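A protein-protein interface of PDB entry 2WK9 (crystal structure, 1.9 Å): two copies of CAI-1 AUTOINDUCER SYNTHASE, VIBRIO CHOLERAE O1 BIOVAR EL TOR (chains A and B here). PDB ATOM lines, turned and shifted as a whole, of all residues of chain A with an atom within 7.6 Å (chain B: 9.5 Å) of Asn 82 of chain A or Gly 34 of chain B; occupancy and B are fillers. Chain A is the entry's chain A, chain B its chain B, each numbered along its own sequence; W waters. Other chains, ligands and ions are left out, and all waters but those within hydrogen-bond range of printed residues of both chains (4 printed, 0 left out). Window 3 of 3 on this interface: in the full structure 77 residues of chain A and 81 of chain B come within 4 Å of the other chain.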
ATOM      1  N   ALA A  77     -14.583 -11.895  14.224  1.00  0.00           N
ATOM      2  CA  ALA A  77     -14.284 -10.760  13.357  1.00  0.00           C
ATOM      3  C   ALA A  77     -15.538  -9.950  13.033  1.00  0.00           C
ATOM      4  O   ALA A  77     -15.455  -8.799  12.606  1.00  0.00           O
ATOM      5  CB  ALA A  77     -13.609 -11.231  12.074  1.00  0.00           C
ATOM      6  N   SER A  78     -16.705 -10.547  13.243  1.00  0.00           N
ATOM      7  CA  SER A  78     -17.949  -9.855  12.936  1.00  0.00           C
ATOM      8  C   SER A  78     -18.064  -8.608  13.805  1.00  0.00           C
ATOM      9  O   SER A  78     -18.598  -7.587  13.368  1.00  0.00           O
ATOM     10  CB  SER A  78     -19.151 -10.777  13.157  1.00  0.00           C
ATOM     11  OG  SER A  78     -19.288 -11.072  14.534  1.00  0.00           O
ATOM     12  N   PHE A  79     -17.541  -8.698  15.028  1.00  0.00           N
ATOM     13  CA  PHE A  79     -17.597  -7.596  15.983  1.00  0.00           C
ATOM     14  C   PHE A  79     -16.574  -6.510  15.656  1.00  0.00           C
ATOM     15  O   PHE A  79     -16.602  -5.431  16.243  1.00  0.00           O
ATOM     16  CB  PHE A  79     -17.361  -8.098  17.417  1.00  0.00           C
ATOM     17  CG  PHE A  79     -18.463  -8.981  17.951  1.00  0.00           C
ATOM     18  CD1 PHE A  79     -19.765  -8.507  18.060  1.00  0.00           C
ATOM     19  CD2 PHE A  79     -18.192 -10.281  18.360  1.00  0.00           C
ATOM     20  CE1 PHE A  79     -20.787  -9.322  18.556  1.00  0.00           C
ATOM     21  CE2 PHE A  79     -19.200 -11.096  18.858  1.00  0.00           C
ATOM     22  CZ  PHE A  79     -20.500 -10.616  18.955  1.00  0.00           C
ATOM     23  N   LEU A  80     -15.671  -6.802  14.724  1.00  0.00           N
ATOM     24  CA  LEU A  80     -14.611  -5.861  14.356  1.00  0.00           C
ATOM     25  C   LEU A  80     -14.764  -5.341  12.930  1.00  0.00           C
ATOM     26  O   LEU A  80     -13.769  -5.144  12.224  1.00  0.00           O
ATOM     27  CB  LEU A  80     -13.239  -6.518  14.513  1.00  0.00           C
ATOM     28  CG  LEU A  80     -12.876  -7.019  15.915  1.00  0.00           C
ATOM     29  CD1 LEU A  80     -11.687  -7.975  15.862  1.00  0.00           C
ATOM     30  CD2 LEU A  80     -12.597  -5.847  16.851  1.00  0.00           C
ATOM     31  N   GLN A  81     -16.002  -5.106  12.509  1.00  0.00           N
ATOM     32  CA  GLN A  81     -16.250  -4.673  11.133  1.00  0.00           C
ATOM     33  C   GLN A  81     -16.482  -3.168  10.975  1.00  0.00           C
ATOM     34  O   GLN A  81     -16.805  -2.703   9.886  1.00  0.00           O
ATOM     35  CB  GLN A  81     -17.391  -5.471  10.490  1.00  0.00           C
ATOM     36  CG  GLN A  81     -17.036  -6.923  10.168  1.00  0.00           C
ATOM     37  CD  GLN A  81     -15.756  -7.061   9.341  1.00  0.00           C
ATOM     38  OE1 GLN A  81     -15.660  -6.544   8.226  1.00  0.00           O
ATOM     39  NE2 GLN A  81     -14.773  -7.779   9.885  1.00  0.00           N
ATOM     40  N   ASN A  82     -16.323  -2.410  12.057  1.00  0.00           N
ATOM     41  CA  ASN A  82     -16.277  -0.956  11.942  1.00  0.00           C
ATOM     42  C   ASN A  82     -15.001  -0.539  11.215  1.00  0.00           C
ATOM     43  O   ASN A  82     -13.978  -1.223  11.306  1.00  0.00           O
ATOM     44  CB  ASN A  82     -16.334  -0.295  13.322  1.00  0.00           C
ATOM     45  CG  ASN A  82     -17.737  -0.280  13.910  1.00  0.00           C
ATOM     46  OD1 ASN A  82     -18.693   0.133  13.254  1.00  0.00           O
ATOM     47  ND2 ASN A  82     -17.859  -0.713  15.160  1.00  0.00           N
ATOM     48  N   ASP A  83     -15.061   0.577  10.493  1.00  0.00           N
ATOM     49  CA  ASP A  83     -13.917   1.073   9.724  1.00  0.00           C
ATOM     50  C   ASP A  83     -12.607   1.015  10.502  1.00  0.00           C
ATOM     51  O   ASP A  83     -11.618   0.449  10.036  1.00  0.00           O
ATOM     52  CB  ASP A  83     -14.156   2.519   9.280  1.00  0.00           C
ATOM     53  CG  ASP A  83     -15.290   2.647   8.285  1.00  0.00           C
ATOM     54  OD1 ASP A  83     -15.660   1.626   7.667  1.00  0.00           O
ATOM     55  OD2 ASP A  83     -15.807   3.773   8.119  1.00  0.00           O
ATOM     56  N   TYR A  84     -12.613   1.612  11.691  1.00  0.00           N
ATOM     57  CA  TYR A  84     -11.408   1.770  12.497  1.00  0.00           C
ATOM     58  C   TYR A  84     -10.855   0.450  13.047  1.00  0.00           C
ATOM     59  O   TYR A  84      -9.742   0.412  13.571  1.00  0.00           O
ATOM     60  CB  TYR A  84     -11.673   2.749  13.648  1.00  0.00           C
ATOM     61  CG  TYR A  84     -12.910   2.418  14.453  1.00  0.00           C
ATOM     62  CD1 TYR A  84     -14.131   3.021  14.172  1.00  0.00           C
ATOM     63  CD2 TYR A  84     -12.859   1.490  15.490  1.00  0.00           C
ATOM     64  CE1 TYR A  84     -15.268   2.713  14.906  1.00  0.00           C
ATOM     65  CE2 TYR A  84     -13.992   1.176  16.228  1.00  0.00           C
ATOM     66  CZ  TYR A  84     -15.190   1.792  15.934  1.00  0.00           C
ATOM     67  OH  TYR A  84     -16.315   1.481  16.663  1.00  0.00           O
ATOM     68  N   ASP A  85     -11.631  -0.624  12.938  1.00  0.00           N
ATOM     69  CA  ASP A  85     -11.187  -1.928  13.429  1.00  0.00           C
ATOM     70  C   ASP A  85     -10.657  -2.823  12.309  1.00  0.00           C
ATOM     71  O   ASP A  85      -9.985  -3.823  12.567  1.00  0.00           O
ATOM     72  CB  ASP A  85     -12.316  -2.638  14.179  1.00  0.00           C
ATOM     73  CG  ASP A  85     -12.552  -2.057  15.562  1.00  0.00           C
ATOM     74  OD1 ASP A  85     -11.633  -1.403  16.103  1.00  0.00           O
ATOM     75  OD2 ASP A  85     -13.653  -2.254  16.111  1.00  0.00           O
ATOM     76  N   LYS A  86     -10.970  -2.465  11.069  1.00  0.00           N
ATOM     77  CA  LYS A  86     -10.530  -3.253   9.921  1.00  0.00           C
ATOM     78  C   LYS A  86      -9.076  -2.946   9.567  1.00  0.00           C
ATOM     79  O   LYS A  86      -8.684  -1.782   9.455  1.00  0.00           O
ATOM     80  CB  LYS A  86     -11.461  -3.041   8.724  1.00  0.00           C
ATOM     81  CG  LYS A  86     -12.849  -3.648   8.920  1.00  0.00           C
ATOM     82  CD  LYS A  86     -13.794  -3.299   7.772  1.00  0.00           C
ATOM     83  CE  LYS A  86     -13.453  -4.065   6.500  1.00  0.00           C
ATOM     84  NZ  LYS A  86     -13.452  -5.542   6.722  1.00  0.00           N
ATOM     85  N   PRO A  87      -8.272  -4.002   9.386  1.00  0.00           N
ATOM     86  CA  PRO A  87      -6.815  -3.930   9.220  1.00  0.00           C
ATOM     87  C   PRO A  87      -6.412  -3.264   7.907  1.00  0.00           C
ATOM     88  O   PRO A  87      -7.030  -3.544   6.881  1.00  0.00           O
ATOM     89  CB  PRO A  87      -6.390  -5.408   9.192  1.00  0.00           C
ATOM     90  CG  PRO A  87      -7.608  -6.199   9.605  1.00  0.00           C
ATOM     91  CD  PRO A  87      -8.780  -5.374   9.229  1.00  0.00           C
ATOM     92  N   PHE A 257     -20.863 -11.184   8.387  1.00  0.00           N
ATOM     93  CA  PHE A 257     -22.043 -11.392   9.215  1.00  0.00           C
ATOM     94  C   PHE A 257     -22.835 -12.621   8.799  1.00  0.00           C
ATOM     95  O   PHE A 257     -23.830 -12.972   9.437  1.00  0.00           O
ATOM     96  CB  PHE A 257     -22.930 -10.146   9.186  1.00  0.00           C
ATOM     97  CG  PHE A 257     -22.176  -8.877   9.448  1.00  0.00           C
ATOM     98  CD1 PHE A 257     -21.825  -8.520  10.736  1.00  0.00           C
ATOM     99  CD2 PHE A 257     -21.795  -8.052   8.402  1.00  0.00           C
ATOM    100  CE1 PHE A 257     -21.125  -7.356  10.979  1.00  0.00           C
ATOM    101  CE2 PHE A 257     -21.091  -6.888   8.639  1.00  0.00           C
ATOM    102  CZ  PHE A 257     -20.757  -6.538   9.928  1.00  0.00           C
ATOM    103  N   ASN B  25     -31.411  -0.816  11.164  1.00  0.00           N
ATOM    104  CA  ASN B  25     -30.810  -0.340  12.401  1.00  0.00           C
ATOM    105  C   ASN B  25     -30.514   1.153  12.345  1.00  0.00           C
ATOM    106  O   ASN B  25     -30.199   1.694  11.285  1.00  0.00           O
ATOM    107  CB  ASN B  25     -29.554  -1.144  12.732  1.00  0.00           C
ATOM    108  CG  ASN B  25     -29.854  -2.616  12.918  1.00  0.00           C
ATOM    109  OD1 ASN B  25     -30.808  -2.983  13.613  1.00  0.00           O
ATOM    110  ND2 ASN B  25     -29.061  -3.468  12.287  1.00  0.00           N
ATOM    111  N   ASN B  27     -28.170   3.062  13.085  1.00  0.00           N
ATOM    112  CA  ASN B  27     -26.881   3.498  12.555  1.00  0.00           C
ATOM    113  C   ASN B  27     -26.595   2.916  11.176  1.00  0.00           C
ATOM    114  O   ASN B  27     -25.492   3.057  10.650  1.00  0.00           O
ATOM    115  CB  ASN B  27     -25.742   3.165  13.526  1.00  0.00           C
ATOM    116  CG  ASN B  27     -25.681   1.688  13.878  1.00  0.00           C
ATOM    117  OD1 ASN B  27     -26.348   0.860  13.260  1.00  0.00           O
ATOM    118  ND2 ASN B  27     -24.881   1.354  14.888  1.00  0.00           N
ATOM    119  N   GLY B  28     -27.595   2.255  10.600  1.00  0.00           N
ATOM    120  CA  GLY B  28     -27.477   1.668   9.280  1.00  0.00           C
ATOM    121  C   GLY B  28     -26.460   0.544   9.176  1.00  0.00           C
ATOM    122  O   GLY B  28     -26.109   0.126   8.071  1.00  0.00           O
ATOM    123  N   LYS B  29     -25.989   0.054  10.320  1.00  0.00           N
ATOM    124  CA  LYS B  29     -24.999  -1.020  10.358  1.00  0.00           C
ATOM    125  C   LYS B  29     -25.611  -2.280  10.954  1.00  0.00           C
ATOM    126  O   LYS B  29     -26.679  -2.234  11.557  1.00  0.00           O
ATOM    127  CB  LYS B  29     -23.794  -0.605  11.203  1.00  0.00           C
ATOM    128  CG  LYS B  29     -23.118   0.683  10.755  1.00  0.00           C
ATOM    129  CD  LYS B  29     -21.877   0.973  11.594  1.00  0.00           C
ATOM    130  CE  LYS B  29     -22.235   1.195  13.058  1.00  0.00           C
ATOM    131  NZ  LYS B  29     -21.076   1.679  13.864  1.00  0.00           N
ATOM    132  N   HIS B  30     -24.935  -3.409  10.787  1.00  0.00           N
ATOM    133  CA  HIS B  30     -25.386  -4.636  11.434  1.00  0.00           C
ATOM    134  C   HIS B  30     -25.555  -4.414  12.936  1.00  0.00           C
ATOM    135  O   HIS B  30     -24.835  -3.619  13.541  1.00  0.00           O
ATOM    136  CB  HIS B  30     -24.390  -5.763  11.186  1.00  0.00           C
ATOM    137  CG  HIS B  30     -24.900  -7.113  11.576  1.00  0.00           C
ATOM    138  ND1 HIS B  30     -24.809  -7.603  12.859  1.00  0.00           N
ATOM    139  CD2 HIS B  30     -25.493  -8.083  10.842  1.00  0.00           C
ATOM    140  CE1 HIS B  30     -25.329  -8.817  12.901  1.00  0.00           C
ATOM    141  NE2 HIS B  30     -25.744  -9.135  11.688  1.00  0.00           N
ATOM    142  N   LEU B  31     -26.503  -5.127  13.531  1.00  0.00           N
ATOM    143  CA  LEU B  31     -26.808  -4.980  14.953  1.00  0.00           C
ATOM    144  C   LEU B  31     -25.607  -5.162  15.899  1.00  0.00           C
ATOM    145  O   LEU B  31     -25.609  -4.630  17.010  1.00  0.00           O
ATOM    146  CB  LEU B  31     -27.928  -5.946  15.348  1.00  0.00           C
ATOM    147  CG  LEU B  31     -28.444  -5.852  16.782  1.00  0.00           C
ATOM    148  CD1 LEU B  31     -29.022  -4.458  17.052  1.00  0.00           C
ATOM    149  CD2 LEU B  31     -29.483  -6.933  17.040  1.00  0.00           C
ATOM    150  N   VAL B  32     -24.591  -5.912  15.481  1.00  0.00           N
ATOM    151  CA  VAL B  32     -23.456  -6.151  16.376  1.00  0.00           C
ATOM    152  C   VAL B  32     -22.557  -4.926  16.489  1.00  0.00           C
ATOM    153  O   VAL B  32     -21.757  -4.813  17.417  1.00  0.00           O
ATOM    154  CB  VAL B  32     -22.615  -7.390  15.976  1.00  0.00           C
ATOM    155  CG1 VAL B  32     -23.474  -8.638  15.997  1.00  0.00           C
ATOM    156  CG2 VAL B  32     -21.946  -7.187  14.625  1.00  0.00           C
ATOM    157  N   LEU B  33     -22.710  -4.006  15.549  1.00  0.00           N
ATOM    158  CA  LEU B  33     -21.841  -2.835  15.467  1.00  0.00           C
ATOM    159  C   LEU B  33     -22.431  -1.651  16.214  1.00  0.00           C
ATOM    160  O   LEU B  33     -23.477  -1.127  15.842  1.00  0.00           O
ATOM    161  CB  LEU B  33     -21.572  -2.462  14.004  1.00  0.00           C
ATOM    162  CG  LEU B  33     -20.283  -2.999  13.376  1.00  0.00           C
ATOM    163  CD1 LEU B  33     -19.901  -4.357  13.948  1.00  0.00           C
ATOM    164  CD2 LEU B  33     -20.380  -3.033  11.843  1.00  0.00           C
ATOM    165  N   GLY B  34     -21.757  -1.239  17.278  1.00  0.00           N
ATOM    166  CA  GLY B  34     -22.211  -0.114  18.065  1.00  0.00           C
ATOM    167  C   GLY B  34     -21.261   1.062  17.989  1.00  0.00           C
ATOM    168  O   GLY B  34     -20.594   1.280  16.978  1.00  0.00           O
ATOM    169  N   LYS B  35     -21.213   1.809  19.087  1.00  0.00           N
ATOM    170  CA  LYS B  35     -20.373   2.988  19.274  1.00  0.00           C
ATOM    171  C   LYS B  35     -18.921   2.582  19.502  1.00  0.00           C
ATOM    172  O   LYS B  35     -18.652   1.492  20.004  1.00  0.00           O
ATOM    173  CB  LYS B  35     -20.863   3.696  20.540  1.00  0.00           C
ATOM    174  CG  LYS B  35     -20.709   5.199  20.591  1.00  0.00           C
ATOM    175  CD  LYS B  35     -21.194   5.698  21.950  1.00  0.00           C
ATOM    176  CE  LYS B  35     -22.009   6.980  21.837  1.00  0.00           C
ATOM    177  NZ  LYS B  35     -22.913   7.165  23.015  1.00  0.00           N
ATOM    178  N   GLN B  36     -17.978   3.458  19.163  1.00  0.00           N
ATOM    179  CA  GLN B  36     -16.588   3.207  19.531  1.00  0.00           C
ATOM    180  C   GLN B  36     -16.375   3.505  21.016  1.00  0.00           C
ATOM    181  O   GLN B  36     -16.846   4.525  21.529  1.00  0.00           O
ATOM    182  CB  GLN B  36     -15.619   4.027  18.675  1.00  0.00           C
ATOM    183  CG  GLN B  36     -14.154   3.647  18.892  1.00  0.00           C
ATOM    184  CD  GLN B  36     -13.200   4.396  17.978  1.00  0.00           C
ATOM    185  OE1 GLN B  36     -13.600   5.306  17.250  1.00  0.00           O
ATOM    186  NE2 GLN B  36     -11.927   4.016  18.014  1.00  0.00           N
ATOM    187  N   ALA B  37     -15.674   2.608  21.704  1.00  0.00           N
ATOM    188  CA  ALA B  37     -15.418   2.769  23.129  1.00  0.00           C
ATOM    189  C   ALA B  37     -14.298   3.768  23.376  1.00  0.00           C
ATOM    190  O   ALA B  37     -13.444   3.987  22.515  1.00  0.00           O
ATOM    191  CB  ALA B  37     -15.071   1.425  23.761  1.00  0.00           C
ATOM    192  N   GLN B  45     -15.917  -7.874  26.262  1.00  0.00           N
ATOM    193  CA  GLN B  45     -16.149  -8.555  24.993  1.00  0.00           C
ATOM    194  C   GLN B  45     -15.153  -9.676  24.719  1.00  0.00           C
ATOM    195  O   GLN B  45     -15.453 -10.619  23.993  1.00  0.00           O
ATOM    196  CB  GLN B  45     -16.128  -7.541  23.849  1.00  0.00           C
ATOM    197  CG  GLN B  45     -17.202  -6.463  23.965  1.00  0.00           C
ATOM    198  CD  GLN B  45     -17.012  -5.341  22.964  1.00  0.00           C
ATOM    199  OE1 GLN B  45     -15.899  -5.091  22.502  1.00  0.00           O
ATOM    200  NE2 GLN B  45     -18.100  -4.665  22.616  1.00  0.00           N
ATOM    201  N   THR B 328     -33.216  -4.964  21.564  1.00  0.00           N
ATOM    202  CA  THR B 328     -31.793  -5.199  21.781  1.00  0.00           C
ATOM    203  C   THR B 328     -30.942  -3.992  21.387  1.00  0.00           C
ATOM    204  O   THR B 328     -29.987  -3.636  22.085  1.00  0.00           O
ATOM    205  CB  THR B 328     -31.344  -6.451  21.014  1.00  0.00           C
ATOM    206  OG1 THR B 328     -31.994  -7.595  21.585  1.00  0.00           O
ATOM    207  CG2 THR B 328     -29.827  -6.624  21.090  1.00  0.00           C
ATOM    208  N   GLU B 329     -31.288  -3.361  20.274  1.00  0.00           N
ATOM    209  CA  GLU B 329     -30.543  -2.193  19.824  1.00  0.00           C
ATOM    210  C   GLU B 329     -30.609  -1.109  20.890  1.00  0.00           C
ATOM    211  O   GLU B 329     -29.597  -0.500  21.248  1.00  0.00           O
ATOM    212  CB  GLU B 329     -31.095  -1.678  18.489  1.00  0.00           C
ATOM    213  CG  GLU B 329     -30.434  -0.403  18.013  1.00  0.00           C
ATOM    214  CD  GLU B 329     -30.997   0.093  16.696  1.00  0.00           C
ATOM    215  OE1 GLU B 329     -32.235   0.053  16.516  1.00  0.00           O
ATOM    216  OE2 GLU B 329     -30.191   0.532  15.845  1.00  0.00           O
ATOM    217  N   ARG B 332     -28.440  -2.071  24.091  1.00  0.00           N
ATOM    218  CA  ARG B 332     -26.997  -1.948  23.973  1.00  0.00           C
ATOM    219  C   ARG B 332     -26.588  -0.497  23.720  1.00  0.00           C
ATOM    220  O   ARG B 332     -25.532  -0.070  24.165  1.00  0.00           O
ATOM    221  CB  ARG B 332     -26.423  -2.935  22.966  1.00  0.00           C
ATOM    222  CG  ARG B 332     -26.545  -2.527  21.551  1.00  0.00           C
ATOM    223  CD  ARG B 332     -25.292  -1.813  21.060  1.00  0.00           C
ATOM    224  NE  ARG B 332     -25.290  -1.848  19.604  1.00  0.00           N
ATOM    225  CZ  ARG B 332     -26.257  -1.322  18.865  1.00  0.00           C
ATOM    226  NH1 ARG B 332     -27.282  -0.723  19.456  1.00  0.00           N
ATOM    227  NH2 ARG B 332     -26.219  -1.408  17.549  1.00  0.00           N
ATOM    228  N   ASP B 333     -27.443   0.269  23.048  1.00  0.00           N
ATOM    229  CA  ASP B 333     -27.196   1.701  22.896  1.00  0.00           C
ATOM    230  C   ASP B 333     -27.181   2.397  24.252  1.00  0.00           C
ATOM    231  O   ASP B 333     -26.378   3.296  24.486  1.00  0.00           O
ATOM    232  CB  ASP B 333     -28.236   2.354  21.980  1.00  0.00           C
ATOM    233  CG  ASP B 333     -27.905   2.186  20.508  1.00  0.00           C
ATOM    234  OD1 ASP B 333     -26.788   1.711  20.194  1.00  0.00           O
ATOM    235  OD2 ASP B 333     -28.763   2.531  19.667  1.00  0.00           O
ATOM    236  N   TYR B 334     -28.071   1.976  25.147  1.00  0.00           N
ATOM    237  CA  TYR B 334     -28.122   2.543  26.487  1.00  0.00           C
ATOM    238  C   TYR B 334     -26.863   2.181  27.259  1.00  0.00           C
ATOM    239  O   TYR B 334     -26.235   3.033  27.880  1.00  0.00           O
ATOM    240  CB  TYR B 334     -29.357   2.048  27.245  1.00  0.00           C
ATOM    241  CG  TYR B 334     -29.475   2.652  28.626  1.00  0.00           C
ATOM    242  CD1 TYR B 334     -30.166   3.842  28.827  1.00  0.00           C
ATOM    243  CD2 TYR B 334     -28.883   2.042  29.726  1.00  0.00           C
ATOM    244  CE1 TYR B 334     -30.273   4.402  30.082  1.00  0.00           C
ATOM    245  CE2 TYR B 334     -28.986   2.594  30.991  1.00  0.00           C
ATOM    246  CZ  TYR B 334     -29.680   3.776  31.161  1.00  0.00           C
ATOM    247  OH  TYR B 334     -29.787   4.337  32.411  1.00  0.00           O
ATOM    248  N   GLU B 336     -23.877   1.182  26.123  1.00  0.00           N
ATOM    249  CA  GLU B 336     -22.692   1.813  25.548  1.00  0.00           C
ATOM    250  C   GLU B 336     -22.636   3.298  25.886  1.00  0.00           C
ATOM    251  O   GLU B 336     -21.583   3.817  26.245  1.00  0.00           O
ATOM    252  CB  GLU B 336     -22.644   1.593  24.042  1.00  0.00           C
ATOM    253  CG  GLU B 336     -22.413   0.144  23.669  1.00  0.00           C
ATOM    254  CD  GLU B 336     -22.134  -0.037  22.197  1.00  0.00           C
ATOM    255  OE1 GLU B 336     -22.270   0.944  21.440  1.00  0.00           O
ATOM    256  OE2 GLU B 336     -21.782  -1.164  21.801  1.00  0.00           O
ATOM    257  N   SER B 337     -23.778   3.970  25.787  1.00  0.00           N
ATOM    258  CA  SER B 337     -23.861   5.384  26.137  1.00  0.00           C
ATOM    259  C   SER B 337     -23.429   5.626  27.577  1.00  0.00           C
ATOM    260  O   SER B 337     -22.952   6.712  27.923  1.00  0.00           O
ATOM    261  CB  SER B 337     -25.280   5.900  25.907  1.00  0.00           C
ATOM    262  OG  SER B 337     -25.492   7.117  26.597  1.00  0.00           O
ATOM    263  N   VAL B 340     -20.663   0.814  29.229  1.00  0.00           N
ATOM    264  CA  VAL B 340     -20.593  -0.633  29.402  1.00  0.00           C
ATOM    265  C   VAL B 340     -20.699  -1.305  28.038  1.00  0.00           C
ATOM    266  O   VAL B 340     -21.679  -1.116  27.330  1.00  0.00           O
ATOM    267  CB  VAL B 340     -21.711  -1.165  30.327  1.00  0.00           C
ATOM    268  CG1 VAL B 340     -21.642  -2.687  30.421  1.00  0.00           C
ATOM    269  CG2 VAL B 340     -21.609  -0.534  31.710  1.00  0.00           C
ATOM    270  N   PHE B 341     -19.686  -2.089  27.683  1.00  0.00           N
ATOM    271  CA  PHE B 341     -19.595  -2.675  26.343  1.00  0.00           C
ATOM    272  C   PHE B 341     -19.553  -4.204  26.351  1.00  0.00           C
ATOM    273  O   PHE B 341     -18.506  -4.802  26.577  1.00  0.00           O
ATOM    274  CB  PHE B 341     -18.371  -2.119  25.605  1.00  0.00           C
ATOM    275  CG  PHE B 341     -18.554  -0.712  25.110  1.00  0.00           C
ATOM    276  CD1 PHE B 341     -18.834  -0.463  23.777  1.00  0.00           C
ATOM    277  CD2 PHE B 341     -18.465   0.361  25.986  1.00  0.00           C
ATOM    278  CE1 PHE B 341     -19.011   0.830  23.320  1.00  0.00           C
ATOM    279  CE2 PHE B 341     -18.646   1.657  25.535  1.00  0.00           C
ATOM    280  CZ  PHE B 341     -18.918   1.890  24.200  1.00  0.00           C
ATOM    281  N   GLY B 342     -20.703  -4.820  26.105  1.00  0.00           N
ATOM    282  CA  GLY B 342     -20.798  -6.259  25.952  1.00  0.00           C
ATOM    283  C   GLY B 342     -20.871  -6.598  24.476  1.00  0.00           C
ATOM    284  O   GLY B 342     -20.642  -5.728  23.629  1.00  0.00           O
ATOM    285  N   SER B 343     -21.181  -7.853  24.159  1.00  0.00           N
ATOM    286  CA  SER B 343     -21.295  -8.275  22.761  1.00  0.00           C
ATOM    287  C   SER B 343     -22.714  -8.701  22.441  1.00  0.00           C
ATOM    288  O   SER B 343     -23.295  -9.526  23.149  1.00  0.00           O
ATOM    289  CB  SER B 343     -20.353  -9.441  22.445  1.00  0.00           C
ATOM    290  OG  SER B 343     -19.006  -9.115  22.716  1.00  0.00           O
ATOM    291  N   VAL B 344     -23.267  -8.136  21.375  1.00  0.00           N
ATOM    292  CA  VAL B 344     -24.589  -8.525  20.914  1.00  0.00           C
ATOM    293  C   VAL B 344     -24.538  -9.888  20.229  1.00  0.00           C
ATOM    294  O   VAL B 344     -23.797 -10.091  19.265  1.00  0.00           O
ATOM    295  CB  VAL B 344     -25.173  -7.499  19.921  1.00  0.00           C
ATOM    296  CG1 VAL B 344     -26.466  -8.028  19.311  1.00  0.00           C
ATOM    297  CG2 VAL B 344     -25.406  -6.149  20.608  1.00  0.00           C
HETATM  298  O   HOH W   1     -18.520   2.593  15.771  1.00  0.00           O
HETATM  299  O   HOH W   2     -18.949  -1.885  17.596  1.00  0.00           O
HETATM  300  O   HOH W   3     -18.843  -4.579  17.515  1.00  0.00           O
HETATM  301  O   HOH W   4     -23.725 -11.835  12.492  1.00  0.00           O
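Of the 12 printed residues of chain A, 6 touch a printed residue of chain B. Hydrophobic or aromatic side chains of chain A within 4 Å of the printed part of chain B: Phe 79, Tyr 84 and Phe 257. Hydrophobic or aromatic side chains of chain B within 4 Å of the printed part of chain A: His 30, Val 32 and Leu 33.
Water W1 lies within hydrogen-bond range of OH of Tyr 84 of chain A (2.6 Å), O of Gly 34 of chain B (2.7 Å), NZ of Lys 29 of chain B (3.3 Å) and ND2 of Asn 82 of chain A (3.4 Å). Water W3 bridges the backbone carbonyl oxygen (O) of Phe 79 of chain A (2.7 Å) and the backbone carbonyl oxygen (O) of Val 32 of chain B (2.9 Å). Water W2 bridges the backbone NH (N) of Gly 34 of chain B and the side-chain amide nitrogen (ND2) of Asn 82 of chain A. Water W4 lies within hydrogen-bond range of the backbone carbonyl oxygen (O) of Phe 257 of chain A (3.3 Å) and a ring nitrogen (NE2) of His 30 of chain B (3.5 Å).
Among the printed residues, merely in contact across the chains: Phe 79 of chain A with Val 344 of chain B, Tyr 84 of chain A with Gln 36 of chain B, Phe 257 of chain A with His 30 of chain B, Asn 82 of chain A with Leu 33 of chain B, Ser 78 of chain A with Leu 33 of chain B, Ser 78 of chain A with Val 32 of chain B, Phe 79 of chain A with Ser 343 of chain B, Phe 79 of chain A with Val 32 of chain B, Phe 257 of chain A with Val 32 of chain B, Asn 82 of chain A with Gly 34 of chain B and Gln 81 of chain A with Leu 33 of chain B.
The side-chain amino group of Lys 29 of chain B lies within hydrogen-bond range of the backbone carbonyl oxygen of Gly 34 of chain B, 3.2 Å away. O of Leu 33 of chain B lies within hydrogen-bond range of NH2 of Arg 332 of chain B. N of Lys 29 of chain B sits close to OD1 of Asn 27 of chain B (3.1 Å). The backbone carbonyl oxygen (O) of Lys 29 of chain B is in hydrogen-bond range of the side-chain amide nitrogen (ND2) of Asn 25 of chain B, at 2.8 Å. The side-chain amide oxygen of Gln 81 of chain A is in hydrogen-bond range of the side-chain amino group of Lys 86 of chain A (2.9 Å). O of Ala 77 of chain A is in hydrogen-bond range of NE2 of Gln 81 of chain A, at 3.0 Å.
No position is printed for both chains. Of the 12 pairs that touch across the chains among the printed residues, none has its exchanged pair printed and touching as well.
OD1 of Asn 82 of chain A is in hydrogen-bond range of NZ of Lys 29 of chain B, 2.9 Å away.
Asn 82 of chain A touches three residues of chain B. Of chain A, only Asn 82 comes within 4 Å of Gly 34 of chain B. No residue of chain B comes within 4 Å of Asp 83 of chain A. No residue of chain B comes within 4 Å of Asp 85 of chain A. Printed residues of chain B within 4 Å of Phe 79 of chain A: Val 32, Ser 343 and Val 344. Of the printed residues of chain B, Gln 81 of chain A touches Leu 33. Printed residues of chain A within 4 Å of Ser 343 of chain B: Phe 79. Ser 337 of chain B touches none of the printed residues of chain A. The nearest residue of chain A that does not touch Gly 34 of chain B is Tyr 84 of chain A (4.3 Å).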
